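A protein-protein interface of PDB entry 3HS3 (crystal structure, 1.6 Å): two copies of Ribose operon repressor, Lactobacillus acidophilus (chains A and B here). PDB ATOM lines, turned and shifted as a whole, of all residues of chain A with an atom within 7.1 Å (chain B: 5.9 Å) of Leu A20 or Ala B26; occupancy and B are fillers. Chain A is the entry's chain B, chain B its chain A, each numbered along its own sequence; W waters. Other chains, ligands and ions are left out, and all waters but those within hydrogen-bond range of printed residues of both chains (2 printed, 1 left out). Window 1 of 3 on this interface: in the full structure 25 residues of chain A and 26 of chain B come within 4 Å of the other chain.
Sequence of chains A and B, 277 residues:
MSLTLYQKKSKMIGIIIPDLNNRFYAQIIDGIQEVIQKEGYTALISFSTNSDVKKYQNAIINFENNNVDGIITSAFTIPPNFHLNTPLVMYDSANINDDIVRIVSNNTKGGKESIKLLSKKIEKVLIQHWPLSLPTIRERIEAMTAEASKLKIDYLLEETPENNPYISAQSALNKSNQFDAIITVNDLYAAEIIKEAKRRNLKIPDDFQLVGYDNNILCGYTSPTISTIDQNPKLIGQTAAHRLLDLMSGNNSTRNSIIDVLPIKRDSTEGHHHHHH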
ATOM      1  N   ILE A  17       1.433  -8.279  16.168  1.00  0.00           N
ATOM      2  CA  ILE A  17       2.309  -9.448  16.064  1.00  0.00           C
ATOM      3  C   ILE A  17       2.795  -9.535  14.621  1.00  0.00           C
ATOM      4  O   ILE A  17       2.192  -8.952  13.726  1.00  0.00           O
ATOM      5  CB  ILE A  17       1.567 -10.768  16.374  1.00  0.00           C
ATOM      6  CG1 ILE A  17       0.372 -10.926  15.431  1.00  0.00           C
ATOM      7  CG2 ILE A  17       1.123 -10.797  17.819  1.00  0.00           C
ATOM      8  CD1 ILE A  17      -0.337 -12.258  15.559  1.00  0.00           C
ATOM      9  N   PRO A  18       3.898 -10.257  14.377  1.00  0.00           N
ATOM     10  CA  PRO A  18       4.413 -10.384  13.007  1.00  0.00           C
ATOM     11  C   PRO A  18       3.505 -11.286  12.171  1.00  0.00           C
ATOM     12  O   PRO A  18       3.081 -10.924  11.072  1.00  0.00           O
ATOM     13  CB  PRO A  18       5.795 -11.003  13.213  1.00  0.00           C
ATOM     14  CG  PRO A  18       6.188 -10.513  14.577  1.00  0.00           C
ATOM     15  CD  PRO A  18       4.908 -10.695  15.356  1.00  0.00           C
ATOM     16  N   ASP A  19       3.222 -12.466  12.710  1.00  0.00           N
ATOM     17  CA  ASP A  19       2.363 -13.455  12.066  1.00  0.00           C
ATOM     18  C   ASP A  19       2.104 -14.578  13.070  1.00  0.00           C
ATOM     19  O   ASP A  19       2.581 -14.523  14.200  1.00  0.00           O
ATOM     20  CB  ASP A  19       3.031 -14.023  10.810  1.00  0.00           C
ATOM     21  CG  ASP A  19       4.394 -14.616  11.092  1.00  0.00           C
ATOM     22  OD1 ASP A  19       5.354 -13.841  11.290  1.00  0.00           O
ATOM     23  OD2 ASP A  19       4.503 -15.859  11.121  1.00  0.00           O
ATOM     24  N   LEU A  20       1.356 -15.598  12.658  1.00  0.00           N
ATOM     25  CA  LEU A  20       1.041 -16.711  13.551  1.00  0.00           C
ATOM     26  C   LEU A  20       1.719 -18.038  13.216  1.00  0.00           C
ATOM     27  O   LEU A  20       1.286 -19.088  13.693  1.00  0.00           O
ATOM     28  CB  LEU A  20      -0.478 -16.933  13.588  1.00  0.00           C
ATOM     29  CG  LEU A  20      -1.357 -15.784  14.076  1.00  0.00           C
ATOM     30  CD1 LEU A  20      -2.816 -16.086  13.778  1.00  0.00           C
ATOM     31  CD2 LEU A  20      -1.134 -15.569  15.562  1.00  0.00           C
ATOM     32  N   ASN A  21       2.771 -18.008  12.402  1.00  0.00           N
ATOM     33  CA  ASN A  21       3.447 -19.243  12.008  1.00  0.00           C
ATOM     34  C   ASN A  21       4.243 -19.940  13.099  1.00  0.00           C
ATOM     35  O   ASN A  21       3.923 -21.065  13.478  1.00  0.00           O
ATOM     36  CB  ASN A  21       4.351 -18.976  10.800  1.00  0.00           C
ATOM     37  CG  ASN A  21       3.618 -19.147   9.489  1.00  0.00           C
ATOM     38  OD1 ASN A  21       3.185 -20.249   9.155  1.00  0.00           O
ATOM     39  ND2 ASN A  21       3.466 -18.061   8.742  1.00  0.00           N
ATOM     40  N   ASN A  22       5.278 -19.269  13.598  1.00  0.00           N
ATOM     41  CA  ASN A  22       6.136 -19.837  14.629  1.00  0.00           C
ATOM     42  C   ASN A  22       5.341 -20.219  15.863  1.00  0.00           C
ATOM     43  O   ASN A  22       4.211 -19.749  16.043  1.00  0.00           O
ATOM     44  CB  ASN A  22       7.209 -18.841  15.027  1.00  0.00           C
ATOM     45  CG  ASN A  22       8.325 -19.488  15.815  1.00  0.00           C
ATOM     46  OD1 ASN A  22       8.808 -20.567  15.449  1.00  0.00           O
ATOM     47  ND2 ASN A  22       8.754 -18.837  16.900  1.00  0.00           N
ATOM     48  N   ARG A  23       5.905 -21.074  16.717  1.00  0.00           N
ATOM     49  CA  ARG A  23       5.220 -21.498  17.953  1.00  0.00           C
ATOM     50  C   ARG A  23       5.125 -20.313  18.913  1.00  0.00           C
ATOM     51  O   ARG A  23       4.116 -20.110  19.578  1.00  0.00           O
ATOM     52  CB  ARG A  23       6.007 -22.648  18.611  1.00  0.00           C
ATOM     53  CG  ARG A  23       5.440 -23.104  19.960  1.00  0.00           C
ATOM     54  CD  ARG A  23       6.127 -24.391  20.417  1.00  0.00           C
ATOM     55  NE  ARG A  23       5.583 -24.900  21.673  1.00  0.00           N
ATOM     56  CZ  ARG A  23       5.907 -24.440  22.880  1.00  0.00           C
ATOM     57  NH1 ARG A  23       6.786 -23.455  23.007  1.00  0.00           N
ATOM     58  NH2 ARG A  23       5.339 -24.957  23.966  1.00  0.00           N
ATOM     59  N   TYR A  25       4.861 -16.886  18.526  1.00  0.00           N
ATOM     60  CA  TYR A  25       3.762 -15.941  18.329  1.00  0.00           C
ATOM     61  C   TYR A  25       2.371 -16.557  18.316  1.00  0.00           C
ATOM     62  O   TYR A  25       1.418 -15.940  18.795  1.00  0.00           O
ATOM     63  CB  TYR A  25       3.993 -15.134  17.050  1.00  0.00           C
ATOM     64  CG  TYR A  25       5.197 -14.233  17.154  1.00  0.00           C
ATOM     65  CD1 TYR A  25       5.222 -13.180  18.066  1.00  0.00           C
ATOM     66  CD2 TYR A  25       6.332 -14.464  16.383  1.00  0.00           C
ATOM     67  CE1 TYR A  25       6.350 -12.380  18.214  1.00  0.00           C
ATOM     68  CE2 TYR A  25       7.469 -13.668  16.523  1.00  0.00           C
ATOM     69  CZ  TYR A  25       7.471 -12.629  17.442  1.00  0.00           C
ATOM     70  OH  TYR A  25       8.604 -11.858  17.601  1.00  0.00           O
ATOM     71  N   ALA A  26       2.242 -17.763  17.771  1.00  0.00           N
ATOM     72  CA  ALA A  26       0.948 -18.438  17.727  1.00  0.00           C
ATOM     73  C   ALA A  26       0.496 -18.742  19.150  1.00  0.00           C
ATOM     74  O   ALA A  26      -0.680 -18.580  19.494  1.00  0.00           O
ATOM     75  CB  ALA A  26       1.058 -19.735  16.927  1.00  0.00           C
ATOM     76  N   GLN A  27       1.436 -19.184  19.980  1.00  0.00           N
ATOM     77  CA  GLN A  27       1.133 -19.505  21.366  1.00  0.00           C
ATOM     78  C   GLN A  27       0.869 -18.248  22.188  1.00  0.00           C
ATOM     79  O   GLN A  27       0.054 -18.266  23.105  1.00  0.00           O
ATOM     80  CB  GLN A  27       2.271 -20.322  21.986  1.00  0.00           C
ATOM     81  CG  GLN A  27       2.256 -21.794  21.584  1.00  0.00           C
ATOM     82  CD  GLN A  27       1.214 -22.609  22.339  1.00  0.00           C
ATOM     83  OE1 GLN A  27       1.389 -22.927  23.518  1.00  0.00           O
ATOM     84  NE2 GLN A  27       0.122 -22.948  21.664  1.00  0.00           N
ATOM     85  N   ILE A  28       1.554 -17.153  21.871  1.00  0.00           N
ATOM     86  CA  ILE A  28       1.315 -15.921  22.611  1.00  0.00           C
ATOM     87  C   ILE A  28      -0.123 -15.482  22.330  1.00  0.00           C
ATOM     88  O   ILE A  28      -0.868 -15.136  23.246  1.00  0.00           O
ATOM     89  CB  ILE A  28       2.326 -14.822  22.212  1.00  0.00           C
ATOM     90  CG1 ILE A  28       3.662 -15.103  22.906  1.00  0.00           C
ATOM     91  CG2 ILE A  28       1.791 -13.436  22.586  1.00  0.00           C
ATOM     92  CD1 ILE A  28       4.816 -14.227  22.457  1.00  0.00           C
ATOM     93  N   ILE A  29      -0.522 -15.526  21.064  1.00  0.00           N
ATOM     94  CA  ILE A  29      -1.887 -15.148  20.703  1.00  0.00           C
ATOM     95  C   ILE A  29      -2.890 -16.111  21.323  1.00  0.00           C
ATOM     96  O   ILE A  29      -3.965 -15.700  21.767  1.00  0.00           O
ATOM     97  CB  ILE A  29      -2.080 -15.139  19.171  1.00  0.00           C
ATOM     98  CG1 ILE A  29      -1.231 -14.024  18.556  1.00  0.00           C
ATOM     99  CG2 ILE A  29      -3.552 -14.934  18.820  1.00  0.00           C
ATOM    100  CD1 ILE A  29      -1.610 -12.630  19.021  1.00  0.00           C
ATOM    101  N   ASP A  30      -2.542 -17.396  21.357  1.00  0.00           N
ATOM    102  CA  ASP A  30      -3.420 -18.405  21.941  1.00  0.00           C
ATOM    103  C   ASP A  30      -3.648 -18.036  23.405  1.00  0.00           C
ATOM    104  O   ASP A  30      -4.777 -18.058  23.891  1.00  0.00           O
ATOM    105  CB  ASP A  30      -2.778 -19.800  21.828  1.00  0.00           C
ATOM    106  CG  ASP A  30      -3.758 -20.936  22.129  1.00  0.00           C
ATOM    107  OD1 ASP A  30      -4.981 -20.685  22.244  1.00  0.00           O
ATOM    108  OD2 ASP A  30      -3.305 -22.091  22.239  1.00  0.00           O
ATOM    109  N   ILE A  45      -6.411  -7.473  15.416  1.00  0.00           N
ATOM    110  CA  ILE A  45      -4.995  -7.710  15.174  1.00  0.00           C
ATOM    111  C   ILE A  45      -4.363  -7.080  13.945  1.00  0.00           C
ATOM    112  O   ILE A  45      -4.861  -7.221  12.830  1.00  0.00           O
ATOM    113  CB  ILE A  45      -4.735  -9.230  15.126  1.00  0.00           C
ATOM    114  CG1 ILE A  45      -5.371  -9.889  16.356  1.00  0.00           C
ATOM    115  CG2 ILE A  45      -3.233  -9.511  15.057  1.00  0.00           C
ATOM    116  CD1 ILE A  45      -5.195 -11.396  16.416  1.00  0.00           C
ATOM    117  N   PHE A  47      -0.897  -6.990  11.775  1.00  0.00           N
ATOM    118  CA  PHE A  47       0.311  -7.764  11.537  1.00  0.00           C
ATOM    119  C   PHE A  47       1.407  -6.869  10.992  1.00  0.00           C
ATOM    120  O   PHE A  47       1.226  -6.203   9.974  1.00  0.00           O
ATOM    121  CB  PHE A  47       0.003  -8.893  10.561  1.00  0.00           C
ATOM    122  CG  PHE A  47      -1.009  -9.868  11.085  1.00  0.00           C
ATOM    123  CD1 PHE A  47      -0.616 -10.926  11.897  1.00  0.00           C
ATOM    124  CD2 PHE A  47      -2.367  -9.702  10.805  1.00  0.00           C
ATOM    125  CE1 PHE A  47      -1.560 -11.810  12.429  1.00  0.00           C
ATOM    126  CE2 PHE A  47      -3.319 -10.580  11.332  1.00  0.00           C
ATOM    127  CZ  PHE A  47      -2.917 -11.635  12.144  1.00  0.00           C
ATOM    128  N   ILE B  17     -10.901 -18.317  12.826  1.00  0.00           N
ATOM    129  CA  ILE B  17      -9.881 -19.346  12.641  1.00  0.00           C
ATOM    130  C   ILE B  17     -10.099 -20.419  13.701  1.00  0.00           C
ATOM    131  O   ILE B  17     -10.213 -20.114  14.891  1.00  0.00           O
ATOM    132  CB  ILE B  17      -8.455 -18.771  12.777  1.00  0.00           C
ATOM    133  CG1 ILE B  17      -7.441 -19.916  12.843  1.00  0.00           C
ATOM    134  CG2 ILE B  17      -8.355 -17.910  14.011  1.00  0.00           C
ATOM    135  CD1 ILE B  17      -6.001 -19.460  12.954  1.00  0.00           C
ATOM    136  N   ASP B  19      -8.043 -23.559  14.298  1.00  0.00           N
ATOM    137  CA  ASP B  19      -6.861 -24.042  15.011  1.00  0.00           C
ATOM    138  C   ASP B  19      -5.666 -23.118  14.813  1.00  0.00           C
ATOM    139  O   ASP B  19      -4.911 -23.244  13.847  1.00  0.00           O
ATOM    140  CB  ASP B  19      -6.487 -25.453  14.560  1.00  0.00           C
ATOM    141  CG  ASP B  19      -5.528 -26.133  15.524  1.00  0.00           C
ATOM    142  OD1 ASP B  19      -4.575 -25.471  15.992  1.00  0.00           O
ATOM    143  OD2 ASP B  19      -5.724 -27.331  15.812  1.00  0.00           O
ATOM    144  N   LEU B  20      -5.502 -22.200  15.757  1.00  0.00           N
ATOM    145  CA  LEU B  20      -4.426 -21.219  15.742  1.00  0.00           C
ATOM    146  C   LEU B  20      -3.019 -21.822  15.719  1.00  0.00           C
ATOM    147  O   LEU B  20      -2.101 -21.264  15.109  1.00  0.00           O
ATOM    148  CB  LEU B  20      -4.580 -20.306  16.965  1.00  0.00           C
ATOM    149  CG  LEU B  20      -3.477 -19.313  17.328  1.00  0.00           C
ATOM    150  CD1 LEU B  20      -3.155 -18.435  16.131  1.00  0.00           C
ATOM    151  CD2 LEU B  20      -3.937 -18.467  18.508  1.00  0.00           C
ATOM    152  N   ASN B  22      -2.064 -24.572  14.275  1.00  0.00           N
ATOM    153  CA  ASN B  22      -1.767 -25.341  13.068  1.00  0.00           C
ATOM    154  C   ASN B  22      -1.179 -24.366  12.057  1.00  0.00           C
ATOM    155  O   ASN B  22      -1.811 -23.364  11.716  1.00  0.00           O
ATOM    156  CB  ASN B  22      -3.042 -25.965  12.492  1.00  0.00           C
ATOM    157  CG  ASN B  22      -2.750 -27.061  11.474  1.00  0.00           C
ATOM    158  OD1 ASN B  22      -1.808 -26.960  10.684  1.00  0.00           O
ATOM    159  ND2 ASN B  22      -3.566 -28.110  11.485  1.00  0.00           N
ATOM    160  N   ARG B  23       0.029 -24.644  11.583  1.00  0.00           N
ATOM    161  CA  ARG B  23       0.662 -23.761  10.614  1.00  0.00           C
ATOM    162  C   ARG B  23      -0.188 -23.603   9.350  1.00  0.00           C
ATOM    163  O   ARG B  23       0.003 -22.667   8.582  1.00  0.00           O
ATOM    164  CB  ARG B  23       2.063 -24.276  10.261  1.00  0.00           C
ATOM    165  CG  ARG B  23       3.121 -23.992  11.338  1.00  0.00           C
ATOM    166  CD  ARG B  23       4.429 -24.736  11.068  1.00  0.00           C
ATOM    167  NE  ARG B  23       5.466 -24.419  12.052  1.00  0.00           N
ATOM    168  CZ  ARG B  23       6.198 -23.306  12.047  1.00  0.00           C
ATOM    169  NH1 ARG B  23       6.015 -22.392  11.105  1.00  0.00           N
ATOM    170  NH2 ARG B  23       7.111 -23.105  12.990  1.00  0.00           N
ATOM    171  N   PHE B  24      -1.131 -24.515   9.136  1.00  0.00           N
ATOM    172  CA  PHE B  24      -1.992 -24.428   7.959  1.00  0.00           C
ATOM    173  C   PHE B  24      -2.854 -23.170   8.047  1.00  0.00           C
ATOM    174  O   PHE B  24      -2.949 -22.393   7.093  1.00  0.00           O
ATOM    175  CB  PHE B  24      -2.884 -25.665   7.874  1.00  0.00           C
ATOM    176  CG  PHE B  24      -3.882 -25.623   6.750  1.00  0.00           C
ATOM    177  CD1 PHE B  24      -3.467 -25.711   5.425  1.00  0.00           C
ATOM    178  CD2 PHE B  24      -5.243 -25.511   7.021  1.00  0.00           C
ATOM    179  CE1 PHE B  24      -4.394 -25.691   4.378  1.00  0.00           C
ATOM    180  CE2 PHE B  24      -6.185 -25.489   5.985  1.00  0.00           C
ATOM    181  CZ  PHE B  24      -5.756 -25.581   4.661  1.00  0.00           C
ATOM    182  N   TYR B  25      -3.487 -22.972   9.198  1.00  0.00           N
ATOM    183  CA  TYR B  25      -4.328 -21.800   9.400  1.00  0.00           C
ATOM    184  C   TYR B  25      -3.492 -20.543   9.582  1.00  0.00           C
ATOM    185  O   TYR B  25      -3.924 -19.447   9.227  1.00  0.00           O
ATOM    186  CB  TYR B  25      -5.251 -22.024  10.597  1.00  0.00           C
ATOM    187  CG  TYR B  25      -6.243 -23.131  10.342  1.00  0.00           C
ATOM    188  CD1 TYR B  25      -7.256 -22.978   9.397  1.00  0.00           C
ATOM    189  CD2 TYR B  25      -6.130 -24.359  10.991  1.00  0.00           C
ATOM    190  CE1 TYR B  25      -8.128 -24.022   9.099  1.00  0.00           C
ATOM    191  CE2 TYR B  25      -6.997 -25.411  10.701  1.00  0.00           C
ATOM    192  CZ  TYR B  25      -7.993 -25.235   9.751  1.00  0.00           C
ATOM    193  OH  TYR B  25      -8.836 -26.282   9.440  1.00  0.00           O
ATOM    194  N   ALA B  26      -2.292 -20.696  10.128  1.00  0.00           N
ATOM    195  CA  ALA B  26      -1.412 -19.550  10.316  1.00  0.00           C
ATOM    196  C   ALA B  26      -1.078 -18.965   8.945  1.00  0.00           C
ATOM    197  O   ALA B  26      -1.066 -17.747   8.758  1.00  0.00           O
ATOM    198  CB  ALA B  26      -0.133 -19.975  11.034  1.00  0.00           C
ATOM    199  N   GLN B  27      -0.814 -19.840   7.980  1.00  0.00           N
ATOM    200  CA  GLN B  27      -0.473 -19.392   6.637  1.00  0.00           C
ATOM    201  C   GLN B  27      -1.682 -18.824   5.894  1.00  0.00           C
ATOM    202  O   GLN B  27      -1.531 -17.933   5.062  1.00  0.00           O
ATOM    203  CB  GLN B  27       0.180 -20.538   5.858  1.00  0.00           C
ATOM    204  CG  GLN B  27       1.480 -20.998   6.516  1.00  0.00           C
ATOM    205  CD  GLN B  27       2.175 -22.122   5.774  1.00  0.00           C
ATOM    206  OE1 GLN B  27       2.826 -21.902   4.751  1.00  0.00           O
ATOM    207  NE2 GLN B  27       2.038 -23.338   6.289  1.00  0.00           N
ATOM    208  N   ILE B  28      -2.877 -19.327   6.195  1.00  0.00           N
ATOM    209  CA  ILE B  28      -4.079 -18.800   5.545  1.00  0.00           C
ATOM    210  C   ILE B  28      -4.294 -17.368   6.033  1.00  0.00           C
ATOM    211  O   ILE B  28      -4.561 -16.467   5.240  1.00  0.00           O
ATOM    212  CB  ILE B  28      -5.332 -19.659   5.853  1.00  0.00           C
ATOM    213  CG1 ILE B  28      -5.248 -20.983   5.081  1.00  0.00           C
ATOM    214  CG2 ILE B  28      -6.602 -18.901   5.456  1.00  0.00           C
ATOM    215  CD1 ILE B  28      -6.394 -21.943   5.341  1.00  0.00           C
ATOM    216  N   ILE B  29      -4.158 -17.152   7.339  1.00  0.00           N
ATOM    217  CA  ILE B  29      -4.320 -15.812   7.891  1.00  0.00           C
ATOM    218  C   ILE B  29      -3.251 -14.869   7.342  1.00  0.00           C
ATOM    219  O   ILE B  29      -3.529 -13.705   7.058  1.00  0.00           O
ATOM    220  CB  ILE B  29      -4.243 -15.823   9.432  1.00  0.00           C
ATOM    221  CG1 ILE B  29      -5.519 -16.439  10.006  1.00  0.00           C
ATOM    222  CG2 ILE B  29      -4.051 -14.406   9.955  1.00  0.00           C
ATOM    223  CD1 ILE B  29      -5.543 -16.494  11.520  1.00  0.00           C
ATOM    224  N   ASP B  30      -2.027 -15.369   7.191  1.00  0.00           N
ATOM    225  CA  ASP B  30      -0.948 -14.550   6.653  1.00  0.00           C
ATOM    226  C   ASP B  30      -1.340 -14.095   5.245  1.00  0.00           C
ATOM    227  O   ASP B  30      -1.109 -12.951   4.862  1.00  0.00           O
ATOM    228  CB  ASP B  30       0.365 -15.352   6.616  1.00  0.00           C
ATOM    229  CG  ASP B  30       1.536 -14.548   6.064  1.00  0.00           C
ATOM    230  OD1 ASP B  30       1.708 -13.382   6.473  1.00  0.00           O
ATOM    231  OD2 ASP B  30       2.296 -15.084   5.227  1.00  0.00           O
ATOM    232  N   GLY B  31      -1.950 -14.997   4.482  1.00  0.00           N
ATOM    233  CA  GLY B  31      -2.375 -14.658   3.136  1.00  0.00           C
ATOM    234  C   GLY B  31      -3.478 -13.618   3.142  1.00  0.00           C
ATOM    235  O   GLY B  31      -3.482 -12.692   2.329  1.00  0.00           O
ATOM    236  N   ILE B  45     -10.294 -10.729  14.592  1.00  0.00           N
ATOM    237  CA  ILE B  45     -10.264 -12.185  14.621  1.00  0.00           C
ATOM    238  C   ILE B  45     -10.848 -12.873  15.843  1.00  0.00           C
ATOM    239  O   ILE B  45     -10.540 -12.522  16.982  1.00  0.00           O
ATOM    240  CB  ILE B  45      -8.811 -12.671  14.438  1.00  0.00           C
ATOM    241  CG1 ILE B  45      -8.213 -12.025  13.183  1.00  0.00           C
ATOM    242  CG2 ILE B  45      -8.763 -14.186  14.322  1.00  0.00           C
ATOM    243  CD1 ILE B  45      -6.748 -12.341  12.959  1.00  0.00           C
ATOM    244  N   PHE B  47     -11.274 -16.593  17.661  1.00  0.00           N
ATOM    245  CA  PHE B  47     -10.703 -17.930  17.700  1.00  0.00           C
ATOM    246  C   PHE B  47     -11.733 -18.890  18.273  1.00  0.00           C
ATOM    247  O   PHE B  47     -12.285 -18.655  19.344  1.00  0.00           O
ATOM    248  CB  PHE B  47      -9.435 -17.895  18.549  1.00  0.00           C
ATOM    249  CG  PHE B  47      -8.403 -16.933  18.031  1.00  0.00           C
ATOM    250  CD1 PHE B  47      -7.442 -17.350  17.112  1.00  0.00           C
ATOM    251  CD2 PHE B  47      -8.418 -15.594  18.422  1.00  0.00           C
ATOM    252  CE1 PHE B  47      -6.509 -16.446  16.585  1.00  0.00           C
ATOM    253  CE2 PHE B  47      -7.494 -14.680  17.904  1.00  0.00           C
ATOM    254  CZ  PHE B  47      -6.537 -15.107  16.984  1.00  0.00           C
HETATM  255  O   HOH W   1       2.839 -17.720   5.955  1.00  0.00           O
HETATM  256  O   HOH W   2       4.665 -22.571   8.376  1.00  0.00           O
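Printed residues of chain B that touch a printed residue of chain A: Leu B20, Arg B23, Ala B26, Gln B27, Ile B29, Ile B45 and Phe B47.
Hydrophobic or aromatic side chains of chain A within 4 Å of the printed part of chain B: Leu A20, Ala A26, Ile A29, Ile A45 and Phe A47.
Along chain A the printed residues that touch a printed residue of chain B span positions 20 to 47.
Among the printed residues, no Asp or Glu carboxylate lies within 4 Å of a Lys or Arg side-chain nitrogen of the other chain.
Water W1 bridges OD2 of Asp B30 (2.8 Å) and ND2 of Asn A21 (2.9 Å).
Water W2 lies within hydrogen-bond range of OD1 of Asn A21 (2.9 Å), NH1 of Arg B23 (3.0 Å) and NE2 of Gln B27 (3.4 Å).
Among the printed residues, merely in contact across the chains: Leu A20 with Leu B20 (3.3 Å), Leu A20 with Ala B26 (3.1 Å), Leu A20 with Ile B29 (3.6 Å), Asn A21 with Ala B26 (3.8 Å), Asn A21 with Gln B27 (3.2 Å), Asn A22 with Arg B23 (3.8 Å), Ala A26 with Leu B20 (3.4 Å), Ile A29 with Leu B20 (3.6 Å), Ile A29 with Phe B47 (3.5 Å), Asp A30 with Leu B20 (3.3 Å), Ile A45 with Ile B45 (3.9 Å), Ile A45 with Phe B47 (3.99 Å), Phe A47 with Ile B29 (3.7 Å) and Phe A47 with Ile B45 (3.98 Å).
NH1 of Arg B23 sits at hydrogen-bond distance from O of Asn A21.
Of the printed residues of chain A, Arg B23 touches Asn A21 and Asn A22.
Of the printed residues of chain A, Ala B26 touches Leu A20 (3.1 Å) and Asn A21 (3.8 Å).
Of the printed residues of chain A, Ile B45 touches Ile A45 (3.9 Å) and Phe A47 (3.98 Å).
The nearest residue of chain B that does not touch Leu A20 is Phe B47 (4.7 Å).
The nearest residue of chain A that does not touch Ala B26 is Asp A19 (5.9 Å).
NE2 of Gln B27 lies close to O of Arg B23 (3.1 Å).
OD2 of Asp A19 lies within hydrogen-bond range of N of Asn A21, 3.0 Å away.
Leu A20 touches its own counterpart, Leu B20.
Leu A20 touches Ala B26, and with the chains exchanged Ala A26 touches Leu B20.
Asn A22 touches Arg B23, but with the chains exchanged Arg A23 does not touch Asn B22 (8.7 Å).
Ile A45 touches its own counterpart, Ile B45.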
